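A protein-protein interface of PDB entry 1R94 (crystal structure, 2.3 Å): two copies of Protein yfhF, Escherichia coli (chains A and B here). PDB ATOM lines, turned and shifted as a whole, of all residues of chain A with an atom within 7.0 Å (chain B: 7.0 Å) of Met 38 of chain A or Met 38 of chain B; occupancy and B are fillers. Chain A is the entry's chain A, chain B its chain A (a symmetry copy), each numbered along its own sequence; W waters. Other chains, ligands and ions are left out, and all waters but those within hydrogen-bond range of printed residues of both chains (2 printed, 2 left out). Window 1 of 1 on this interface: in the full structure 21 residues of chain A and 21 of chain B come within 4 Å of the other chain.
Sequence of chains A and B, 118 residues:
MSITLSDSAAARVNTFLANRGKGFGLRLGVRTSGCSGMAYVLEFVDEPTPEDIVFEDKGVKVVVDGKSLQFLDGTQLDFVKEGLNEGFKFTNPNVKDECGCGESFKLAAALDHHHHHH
The backbone carbonyl oxygen (O) of Ser 36 of chain A is in hydrogen-bond range of the backbone NH (N) of Tyr 40 of chain B (2.9 Å).
The backbone NH (N) of Met 38 of chain A lies within hydrogen-bond range of the backbone carbonyl oxygen (O) of Met 38 of chain B.
N of Tyr 40 of chain A lies within hydrogen-bond range of O of Ser 36 of chain B (2.9 Å).
Of chain B, only Gly 37, Met 38, Tyr 40 and Val 95 come within 4 Å of Met 38 of chain A.
Met 38 of chain B touches just these residues of chain A: Gly 37, Met 38, Tyr 40 and Val 95.
Printed residues of chain A within 4 Å of Gly 37 of chain B: Met 38 and Tyr 40.
Of the printed residues of chain B, Thr 32 of chain A touches Val 95.
The nearest residue of chain B that does not touch Met 38 of chain A is Ser 36 of chain B (4.4 Å).
The nearest residue of chain A that does not touch Met 38 of chain B is Ser 36 of chain A (4.4 Å).
O of Arg 31 of chain A is in hydrogen-bond range of N of Ala 39 of chain A, at 2.5 Å.
The backbone carbonyl oxygen (O) of Arg 31 of chain B is in hydrogen-bond range of the backbone NH (N) of Ala 39 of chain B, at 2.5 Å.
Water W2 bridges the side-chain hydroxyl (OG) of Ser 36 of chain A (2.7 Å) and the backbone carbonyl oxygen (O) of Tyr 40 of chain B (2.7 Å).
Water W1 lies within hydrogen-bond range of OG of Ser 36 of chain B (2.7 Å) and O of Tyr 40 of chain A (2.7 Å).
Among the printed residues, merely in contact across the chains: Val 30 of chain A with Val 95 of chain B, Thr 32 of chain A with Val 95 of chain B, Ser 36 of chain A with Ala 39 of chain B, Ser 36 of chain A with Phe 90 of chain B, Gly 37 of chain A with Met 38 of chain B, Gly 37 of chain A with Tyr 40 of chain B, Met 38 of chain A with Gly 37 of chain B, Met 38 of chain A with Tyr 40 of chain B, Met 38 of chain A with Val 95 of chain B, Ala 39 of chain A with Ser 36 of chain B, Tyr 40 of chain A with Gly 37 of chain B, Tyr 40 of chain A with Met 38 of chain B, Phe 71 of chain A with Phe 71 of chain B, Phe 71 of chain A with Asn 92 of chain B, Phe 71 of chain A with Val 95 of chain B, Phe 90 of chain A with Ser 36 of chain B, Asn 92 of chain A with Phe 71 of chain B, Val 95 of chain A with Val 30 of chain B, Val 95 of chain A with Thr 32 of chain B, Val 95 of chain A with Met 38 of chain B and Val 95 of chain A with Phe 71 of chain B.
Ser 36 of chain A touches Ala 39 of chain B, and with the chains exchanged Ala 39 of chain A touches Ser 36 of chain B.
Ser 36 of chain A touches Phe 90 of chain B, and with the chains exchanged Phe 90 of chain A touches Ser 36 of chain B.
Met 38 of chain A touches Val 95 of chain B, and with the chains exchanged Val 95 of chain A touches Met 38 of chain B.
Phe 71 of chain A touches Asn 92 of chain B, and with the chains exchanged Asn 92 of chain A touches Phe 71 of chain B.
16 positions are printed for both chains.
Of the 24 pairs that touch across the chains among the printed residues, 24 have their exchanged pair printed and touching as well.
Of the 16 printed residues of chain B, 11 touch a printed residue of chain A.
Along chain B the printed residues that touch a printed residue of chain A span positions 30 to 95.
Hydrophobic or aromatic side chains of chain A within 4 Å of the printed part of chain B: Val 30, Met 38, Tyr 40, Phe 71, Phe 90 and Val 95.
Among the printed residues, 24 pairs touch across the chains.
Among the printed residues, no Asp or Glu carboxylate lies within 4 Å of a Lys or Arg side-chain nitrogen of the other chain.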
ATOM      1  N   GLY A  29      16.558 -17.317 -31.349  1.00  0.00           N
ATOM      2  CA  GLY A  29      17.046 -16.046 -30.851  1.00  0.00           C
ATOM      3  C   GLY A  29      15.936 -15.239 -30.183  1.00  0.00           C
ATOM      4  O   GLY A  29      14.767 -15.638 -30.108  1.00  0.00           O
ATOM      5  N   VAL A  30      16.315 -14.063 -29.714  1.00  0.00           N
ATOM      6  CA  VAL A  30      15.419 -13.226 -28.938  1.00  0.00           C
ATOM      7  C   VAL A  30      15.766 -11.789 -29.326  1.00  0.00           C
ATOM      8  O   VAL A  30      16.888 -11.517 -29.750  1.00  0.00           O
ATOM      9  CB  VAL A  30      15.626 -13.545 -27.442  1.00  0.00           C
ATOM     10  CG1 VAL A  30      15.906 -12.317 -26.655  1.00  0.00           C
ATOM     11  CG2 VAL A  30      14.475 -14.334 -26.887  1.00  0.00           C
ATOM     12  N   ARG A  31      14.793 -10.890 -29.262  1.00  0.00           N
ATOM     13  CA  ARG A  31      15.021  -9.474 -29.546  1.00  0.00           C
ATOM     14  C   ARG A  31      13.937  -8.637 -28.862  1.00  0.00           C
ATOM     15  O   ARG A  31      12.853  -9.138 -28.543  1.00  0.00           O
ATOM     16  CB  ARG A  31      15.066  -9.181 -31.065  1.00  0.00           C
ATOM     17  CG  ARG A  31      13.747  -9.452 -31.808  1.00  0.00           C
ATOM     18  CD  ARG A  31      13.658  -8.927 -33.264  1.00  0.00           C
ATOM     19  NE  ARG A  31      12.585  -7.925 -33.360  1.00  0.00           N
ATOM     20  CZ  ARG A  31      11.325  -8.159 -33.759  1.00  0.00           C
ATOM     21  NH1 ARG A  31      10.938  -9.372 -34.157  1.00  0.00           N
ATOM     22  NH2 ARG A  31      10.453  -7.156 -33.769  1.00  0.00           N
ATOM     23  N   THR A  32      14.229  -7.362 -28.640  1.00  0.00           N
ATOM     24  CA  THR A  32      13.219  -6.472 -28.077  1.00  0.00           C
ATOM     25  C   THR A  32      12.116  -6.232 -29.091  1.00  0.00           C
ATOM     26  O   THR A  32      12.362  -6.170 -30.307  1.00  0.00           O
ATOM     27  CB  THR A  32      13.821  -5.105 -27.688  1.00  0.00           C
ATOM     28  OG1 THR A  32      14.289  -4.460 -28.879  1.00  0.00           O
ATOM     29  CG2 THR A  32      15.077  -5.261 -26.817  1.00  0.00           C
ATOM     30  N   SER A  33      10.903  -6.109 -28.576  1.00  0.00           N
ATOM     31  CA  SER A  33       9.784  -5.601 -29.333  1.00  0.00           C
ATOM     32  C   SER A  33       9.164  -4.532 -28.417  1.00  0.00           C
ATOM     33  O   SER A  33       8.313  -4.835 -27.564  1.00  0.00           O
ATOM     34  CB  SER A  33       8.808  -6.739 -29.691  1.00  0.00           C
ATOM     35  OG  SER A  33       7.448  -6.309 -29.764  1.00  0.00           O
ATOM     36  N   GLY A  34       9.647  -3.291 -28.567  1.00  0.00           N
ATOM     37  CA  GLY A  34       9.085  -2.143 -27.866  1.00  0.00           C
ATOM     38  C   GLY A  34       9.810  -1.819 -26.572  1.00  0.00           C
ATOM     39  O   GLY A  34      11.015  -2.095 -26.411  1.00  0.00           O
ATOM     40  N   SER A  36       8.490  -2.636 -23.326  1.00  0.00           N
ATOM     41  CA  SER A  36       8.262  -3.667 -22.337  1.00  0.00           C
ATOM     42  C   SER A  36       7.930  -5.017 -22.986  1.00  0.00           C
ATOM     43  O   SER A  36       7.025  -5.729 -22.530  1.00  0.00           O
ATOM     44  CB  SER A  36       7.172  -3.205 -21.369  1.00  0.00           C
ATOM     45  OG  SER A  36       6.004  -2.870 -22.090  1.00  0.00           O
ATOM     46  N   GLY A  37       8.675  -5.380 -24.033  1.00  0.00           N
ATOM     47  CA  GLY A  37       8.386  -6.591 -24.794  1.00  0.00           C
ATOM     48  C   GLY A  37       9.565  -7.319 -25.435  1.00  0.00           C
ATOM     49  O   GLY A  37      10.611  -6.742 -25.670  1.00  0.00           O
ATOM     50  N   MET A  38       9.371  -8.605 -25.729  1.00  0.00           N
ATOM     51  CA  MET A  38      10.392  -9.441 -26.346  1.00  0.00           C
ATOM     52  C   MET A  38       9.823 -10.185 -27.559  1.00  0.00           C
ATOM     53  O   MET A  38       8.667 -10.602 -27.562  1.00  0.00           O
ATOM     54  CB  MET A  38      10.947 -10.422 -25.310  1.00  0.00           C
ATOM     55  CG  MET A  38      12.283 -11.079 -25.709  1.00  0.00           C
ATOM     56  SD  MET A  38      13.596 -11.108 -24.381  1.00  0.00           S
ATOM     57  CE  MET A  38      13.584  -9.350 -23.808  1.00  0.00           C
ATOM     58  N   ALA A  39      10.617 -10.337 -28.604  1.00  0.00           N
ATOM     59  CA  ALA A  39      10.200 -11.189 -29.716  1.00  0.00           C
ATOM     60  C   ALA A  39      11.169 -12.347 -29.942  1.00  0.00           C
ATOM     61  O   ALA A  39      12.372 -12.148 -29.986  1.00  0.00           O
ATOM     62  CB  ALA A  39      10.014 -10.377 -30.991  1.00  0.00           C
ATOM     63  N   TYR A  40      10.607 -13.545 -30.075  1.00  0.00           N
ATOM     64  CA  TYR A  40      11.334 -14.756 -30.440  1.00  0.00           C
ATOM     65  C   TYR A  40      11.711 -14.701 -31.895  1.00  0.00           C
ATOM     66  O   TYR A  40      10.971 -14.165 -32.696  1.00  0.00           O
ATOM     67  CB  TYR A  40      10.435 -15.945 -30.252  1.00  0.00           C
ATOM     68  CG  TYR A  40      10.152 -16.324 -28.821  1.00  0.00           C
ATOM     69  CD1 TYR A  40       8.963 -15.948 -28.183  1.00  0.00           C
ATOM     70  CD2 TYR A  40      11.054 -17.115 -28.111  1.00  0.00           C
ATOM     71  CE1 TYR A  40       8.687 -16.328 -26.847  1.00  0.00           C
ATOM     72  CE2 TYR A  40      10.785 -17.517 -26.777  1.00  0.00           C
ATOM     73  CZ  TYR A  40       9.600 -17.114 -26.159  1.00  0.00           C
ATOM     74  OH  TYR A  40       9.379 -17.541 -24.859  1.00  0.00           O
ATOM     75  N   PHE A  71      16.656 -16.589 -21.354  1.00  0.00           N
ATOM     76  CA  PHE A  71      15.297 -16.337 -21.836  1.00  0.00           C
ATOM     77  C   PHE A  71      14.641 -17.481 -22.629  1.00  0.00           C
ATOM     78  O   PHE A  71      13.443 -17.405 -22.897  1.00  0.00           O
ATOM     79  CB  PHE A  71      15.195 -15.067 -22.702  1.00  0.00           C
ATOM     80  CG  PHE A  71      16.200 -13.994 -22.362  1.00  0.00           C
ATOM     81  CD1 PHE A  71      17.411 -13.908 -23.049  1.00  0.00           C
ATOM     82  CD2 PHE A  71      15.920 -13.039 -21.369  1.00  0.00           C
ATOM     83  CE1 PHE A  71      18.349 -12.903 -22.732  1.00  0.00           C
ATOM     84  CE2 PHE A  71      16.853 -12.023 -21.053  1.00  0.00           C
ATOM     85  CZ  PHE A  71      18.065 -11.965 -21.715  1.00  0.00           C
ATOM     86  N   THR A  75      11.446 -23.652 -23.380  1.00  0.00           N
ATOM     87  CA  THR A  75      10.624 -23.440 -24.571  1.00  0.00           C
ATOM     88  C   THR A  75      10.355 -24.746 -25.310  1.00  0.00           C
ATOM     89  O   THR A  75      11.267 -25.517 -25.555  1.00  0.00           O
ATOM     90  CB  THR A  75      11.315 -22.456 -25.515  1.00  0.00           C
ATOM     91  OG1 THR A  75      11.211 -21.141 -24.964  1.00  0.00           O
ATOM     92  CG2 THR A  75      10.564 -22.326 -26.824  1.00  0.00           C
ATOM     93  N   PHE A  90       5.840 -20.627 -29.805  1.00  0.00           N
ATOM     94  CA  PHE A  90       6.706 -20.873 -28.674  1.00  0.00           C
ATOM     95  C   PHE A  90       5.863 -20.885 -27.433  1.00  0.00           C
ATOM     96  O   PHE A  90       5.068 -19.994 -27.178  1.00  0.00           O
ATOM     97  CB  PHE A  90       7.756 -19.799 -28.542  1.00  0.00           C
ATOM     98  CG  PHE A  90       8.593 -19.620 -29.741  1.00  0.00           C
ATOM     99  CD1 PHE A  90       8.046 -19.223 -30.941  1.00  0.00           C
ATOM    100  CD2 PHE A  90       9.954 -19.808 -29.664  1.00  0.00           C
ATOM    101  CE1 PHE A  90       8.858 -19.024 -32.068  1.00  0.00           C
ATOM    102  CE2 PHE A  90      10.768 -19.615 -30.784  1.00  0.00           C
ATOM    103  CZ  PHE A  90      10.211 -19.221 -31.982  1.00  0.00           C
ATOM    104  N   ASN A  92       5.997 -22.047 -23.161  1.00  0.00           N
ATOM    105  CA  ASN A  92       6.832 -22.290 -22.014  1.00  0.00           C
ATOM    106  C   ASN A  92       5.847 -22.555 -20.889  1.00  0.00           C
ATOM    107  O   ASN A  92       4.897 -21.782 -20.723  1.00  0.00           O
ATOM    108  CB  ASN A  92       7.733 -21.089 -21.721  1.00  0.00           C
ATOM    109  CG  ASN A  92       8.906 -21.447 -20.838  1.00  0.00           C
ATOM    110  OD1 ASN A  92       8.738 -22.039 -19.769  1.00  0.00           O
ATOM    111  ND2 ASN A  92      10.109 -21.091 -21.282  1.00  0.00           N
ATOM    112  N   VAL A  95       5.190 -19.686 -18.162  1.00  0.00           N
ATOM    113  CA  VAL A  95       4.723 -18.400 -18.711  1.00  0.00           C
ATOM    114  C   VAL A  95       3.214 -18.492 -19.057  1.00  0.00           C
ATOM    115  O   VAL A  95       2.751 -19.508 -19.602  1.00  0.00           O
ATOM    116  CB  VAL A  95       5.567 -17.978 -19.946  1.00  0.00           C
ATOM    117  CG1 VAL A  95       4.935 -16.816 -20.681  1.00  0.00           C
ATOM    118  CG2 VAL A  95       6.960 -17.591 -19.532  1.00  0.00           C
ATOM    119  N   GLY B  29       6.729  -9.121 -13.683  1.00  0.00           N
ATOM    120  CA  GLY B  29       6.182 -10.345 -14.236  1.00  0.00           C
ATOM    121  C   GLY B  29       6.387 -10.422 -15.746  1.00  0.00           C
ATOM    122  O   GLY B  29       6.938  -9.524 -16.396  1.00  0.00           O
ATOM    123  N   VAL B  30       5.902 -11.512 -16.314  1.00  0.00           N
ATOM    124  CA  VAL B  30       6.123 -11.805 -17.717  1.00  0.00           C
ATOM    125  C   VAL B  30       4.844 -12.489 -18.197  1.00  0.00           C
ATOM    126  O   VAL B  30       4.126 -13.088 -17.397  1.00  0.00           O
ATOM    127  CB  VAL B  30       7.392 -12.675 -17.841  1.00  0.00           C
ATOM    128  CG1 VAL B  30       7.129 -13.919 -18.612  1.00  0.00           C
ATOM    129  CG2 VAL B  30       8.544 -11.888 -18.394  1.00  0.00           C
ATOM    130  N   ARG B  31       4.515 -12.338 -19.473  1.00  0.00           N
ATOM    131  CA  ARG B  31       3.350 -12.999 -20.061  1.00  0.00           C
ATOM    132  C   ARG B  31       3.542 -13.117 -21.575  1.00  0.00           C
ATOM    133  O   ARG B  31       4.321 -12.370 -22.178  1.00  0.00           O
ATOM    134  CB  ARG B  31       2.030 -12.263 -19.728  1.00  0.00           C
ATOM    135  CG  ARG B  31       1.925 -10.844 -20.310  1.00  0.00           C
ATOM    136  CD  ARG B  31       0.530 -10.171 -20.236  1.00  0.00           C
ATOM    137  NE  ARG B  31       0.037  -9.910 -21.597  1.00  0.00           N
ATOM    138  CZ  ARG B  31       0.151  -8.752 -22.265  1.00  0.00           C
ATOM    139  NH1 ARG B  31       0.713  -7.680 -21.703  1.00  0.00           N
ATOM    140  NH2 ARG B  31      -0.320  -8.671 -23.505  1.00  0.00           N
ATOM    141  N   THR B  32       2.830 -14.051 -22.189  1.00  0.00           N
ATOM    142  CA  THR B  32       2.882 -14.170 -23.642  1.00  0.00           C
ATOM    143  C   THR B  32       2.205 -12.974 -24.284  1.00  0.00           C
ATOM    144  O   THR B  32       1.216 -12.436 -23.761  1.00  0.00           O
ATOM    145  CB  THR B  32       2.170 -15.448 -24.133  1.00  0.00           C
ATOM    146  OG1 THR B  32       0.780 -15.349 -23.800  1.00  0.00           O
ATOM    147  CG2 THR B  32       2.656 -16.698 -23.383  1.00  0.00           C
ATOM    148  N   SER B  33       2.756 -12.563 -25.415  1.00  0.00           N
ATOM    149  CA  SER B  33       2.100 -11.639 -26.310  1.00  0.00           C
ATOM    150  C   SER B  33       2.220 -12.305 -27.693  1.00  0.00           C
ATOM    151  O   SER B  33       3.219 -12.122 -28.407  1.00  0.00           O
ATOM    152  CB  SER B  33       2.765 -10.250 -26.242  1.00  0.00           C
ATOM    153  OG  SER B  33       2.715  -9.543 -27.481  1.00  0.00           O
ATOM    154  N   GLY B  34       1.214 -13.124 -28.028  1.00  0.00           N
ATOM    155  CA  GLY B  34       1.112 -13.736 -29.347  1.00  0.00           C
ATOM    156  C   GLY B  34       1.713 -15.129 -29.408  1.00  0.00           C
ATOM    157  O   GLY B  34       1.761 -15.865 -28.402  1.00  0.00           O
ATOM    158  N   SER B  36       4.908 -15.825 -30.909  1.00  0.00           N
ATOM    159  CA  SER B  36       6.347 -15.771 -30.771  1.00  0.00           C
ATOM    160  C   SER B  36       6.801 -14.519 -30.009  1.00  0.00           C
ATOM    161  O   SER B  36       7.780 -13.867 -30.395  1.00  0.00           O
ATOM    162  CB  SER B  36       6.990 -15.872 -32.154  1.00  0.00           C
ATOM    163  OG  SER B  36       6.482 -14.856 -32.993  1.00  0.00           O
ATOM    164  N   GLY B  37       6.106 -14.197 -28.915  1.00  0.00           N
ATOM    165  CA  GLY B  37       6.379 -12.973 -28.168  1.00  0.00           C
ATOM    166  C   GLY B  37       6.130 -12.995 -26.662  1.00  0.00           C
ATOM    167  O   GLY B  37       5.371 -13.804 -26.161  1.00  0.00           O
ATOM    168  N   MET B  38       6.776 -12.074 -25.948  1.00  0.00           N
ATOM    169  CA  MET B  38       6.646 -11.956 -24.501  1.00  0.00           C
ATOM    170  C   MET B  38       6.343 -10.509 -24.101  1.00  0.00           C
ATOM    171  O   MET B  38       6.845  -9.565 -24.705  1.00  0.00           O
ATOM    172  CB  MET B  38       7.927 -12.456 -23.829  1.00  0.00           C
ATOM    173  CG  MET B  38       7.779 -12.758 -22.324  1.00  0.00           C
ATOM    174  SD  MET B  38       8.510 -14.377 -21.750  1.00  0.00           S
ATOM    175  CE  MET B  38       7.809 -15.561 -22.986  1.00  0.00           C
ATOM    176  N   ALA B  39       5.504 -10.321 -23.096  1.00  0.00           N
ATOM    177  CA  ALA B  39       5.314  -8.979 -22.550  1.00  0.00           C
ATOM    178  C   ALA B  39       5.690  -8.906 -21.072  1.00  0.00           C
ATOM    179  O   ALA B  39       5.283  -9.747 -20.288  1.00  0.00           O
ATOM    180  CB  ALA B  39       3.889  -8.491 -22.774  1.00  0.00           C
ATOM    181  N   TYR B  40       6.475  -7.888 -20.731  1.00  0.00           N
ATOM    182  CA  TYR B  40       6.832  -7.552 -19.358  1.00  0.00           C
ATOM    183  C   TYR B  40       5.643  -6.952 -18.658  1.00  0.00           C
ATOM    184  O   TYR B  40       4.860  -6.258 -19.276  1.00  0.00           O
ATOM    185  CB  TYR B  40       7.918  -6.513 -19.372  1.00  0.00           C
ATOM    186  CG  TYR B  40       9.277  -7.002 -19.801  1.00  0.00           C
ATOM    187  CD1 TYR B  40       9.752  -6.802 -21.104  1.00  0.00           C
ATOM    188  CD2 TYR B  40      10.124  -7.623 -18.884  1.00  0.00           C
ATOM    189  CE1 TYR B  40      11.040  -7.239 -21.498  1.00  0.00           C
ATOM    190  CE2 TYR B  40      11.423  -8.051 -19.259  1.00  0.00           C
ATOM    191  CZ  TYR B  40      11.865  -7.855 -20.568  1.00  0.00           C
ATOM    192  OH  TYR B  40      13.146  -8.283 -20.882  1.00  0.00           O
ATOM    193  N   PHE B  71      13.634 -15.499 -17.161  1.00  0.00           N
ATOM    194  CA  PHE B  71      13.394 -14.461 -18.166  1.00  0.00           C
ATOM    195  C   PHE B  71      13.676 -13.015 -17.721  1.00  0.00           C
ATOM    196  O   PHE B  71      13.676 -12.124 -18.570  1.00  0.00           O
ATOM    197  CB  PHE B  71      11.961 -14.493 -18.729  1.00  0.00           C
ATOM    198  CG  PHE B  71      11.318 -15.857 -18.732  1.00  0.00           C
ATOM    199  CD1 PHE B  71      10.506 -16.266 -17.673  1.00  0.00           C
ATOM    200  CD2 PHE B  71      11.499 -16.732 -19.818  1.00  0.00           C
ATOM    201  CE1 PHE B  71       9.904 -17.542 -17.679  1.00  0.00           C
ATOM    202  CE2 PHE B  71      10.889 -18.010 -19.833  1.00  0.00           C
ATOM    203  CZ  PHE B  71      10.113 -18.419 -18.765  1.00  0.00           C
ATOM    204  N   THR B  75      17.733  -7.539 -16.169  1.00  0.00           N
ATOM    205  CA  THR B  75      16.885  -6.404 -16.532  1.00  0.00           C
ATOM    206  C   THR B  75      17.231  -5.160 -15.721  1.00  0.00           C
ATOM    207  O   THR B  75      17.357  -5.226 -14.510  1.00  0.00           O
ATOM    208  CB  THR B  75      15.414  -6.759 -16.314  1.00  0.00           C
ATOM    209  OG1 THR B  75      15.000  -7.656 -17.347  1.00  0.00           O
ATOM    210  CG2 THR B  75      14.517  -5.560 -16.538  1.00  0.00           C
ATOM    211  N   PHE B  90      12.194  -1.573 -20.116  1.00  0.00           N
ATOM    212  CA  PHE B  90      13.010  -2.685 -19.682  1.00  0.00           C
ATOM    213  C   PHE B  90      14.109  -2.879 -20.685  1.00  0.00           C
ATOM    214  O   PHE B  90      13.889  -2.952 -21.884  1.00  0.00           O
ATOM    215  CB  PHE B  90      12.203  -3.954 -19.587  1.00  0.00           C
ATOM    216  CG  PHE B  90      11.029  -3.863 -18.701  1.00  0.00           C
ATOM    217  CD1 PHE B  90      10.001  -2.988 -18.968  1.00  0.00           C
ATOM    218  CD2 PHE B  90      10.928  -4.690 -17.606  1.00  0.00           C
ATOM    219  CE1 PHE B  90       8.873  -2.931 -18.135  1.00  0.00           C
ATOM    220  CE2 PHE B  90       9.809  -4.637 -16.771  1.00  0.00           C
ATOM    221  CZ  PHE B  90       8.785  -3.756 -17.044  1.00  0.00           C
ATOM    222  N   ASN B  92      17.985  -4.951 -21.225  1.00  0.00           N
ATOM    223  CA  ASN B  92      18.817  -6.054 -20.819  1.00  0.00           C
ATOM    224  C   ASN B  92      20.021  -5.966 -21.741  1.00  0.00           C
ATOM    225  O   ASN B  92      19.844  -5.829 -22.956  1.00  0.00           O
ATOM    226  CB  ASN B  92      18.079  -7.386 -20.961  1.00  0.00           C
ATOM    227  CG  ASN B  92      18.721  -8.492 -20.156  1.00  0.00           C
ATOM    228  OD1 ASN B  92      19.925  -8.736 -20.260  1.00  0.00           O
ATOM    229  ND2 ASN B  92      17.917  -9.170 -19.339  1.00  0.00           N
ATOM    230  N   VAL B  95      20.334  -8.556 -24.788  1.00  0.00           N
ATOM    231  CA  VAL B  95      19.200  -8.551 -25.730  1.00  0.00           C
ATOM    232  C   VAL B  95      19.313  -7.333 -26.683  1.00  0.00           C
ATOM    233  O   VAL B  95      19.655  -6.220 -26.249  1.00  0.00           O
ATOM    234  CB  VAL B  95      17.842  -8.559 -24.972  1.00  0.00           C
ATOM    235  CG1 VAL B  95      16.683  -8.276 -25.904  1.00  0.00           C
ATOM    236  CG2 VAL B  95      17.615  -9.885 -24.302  1.00  0.00           C
HETATM  237  O   HOH W   1       8.487 -13.099 -33.041  1.00  0.00           O
HETATM  238  O   HOH W   2       4.431  -4.975 -21.641  1.00  0.00           O
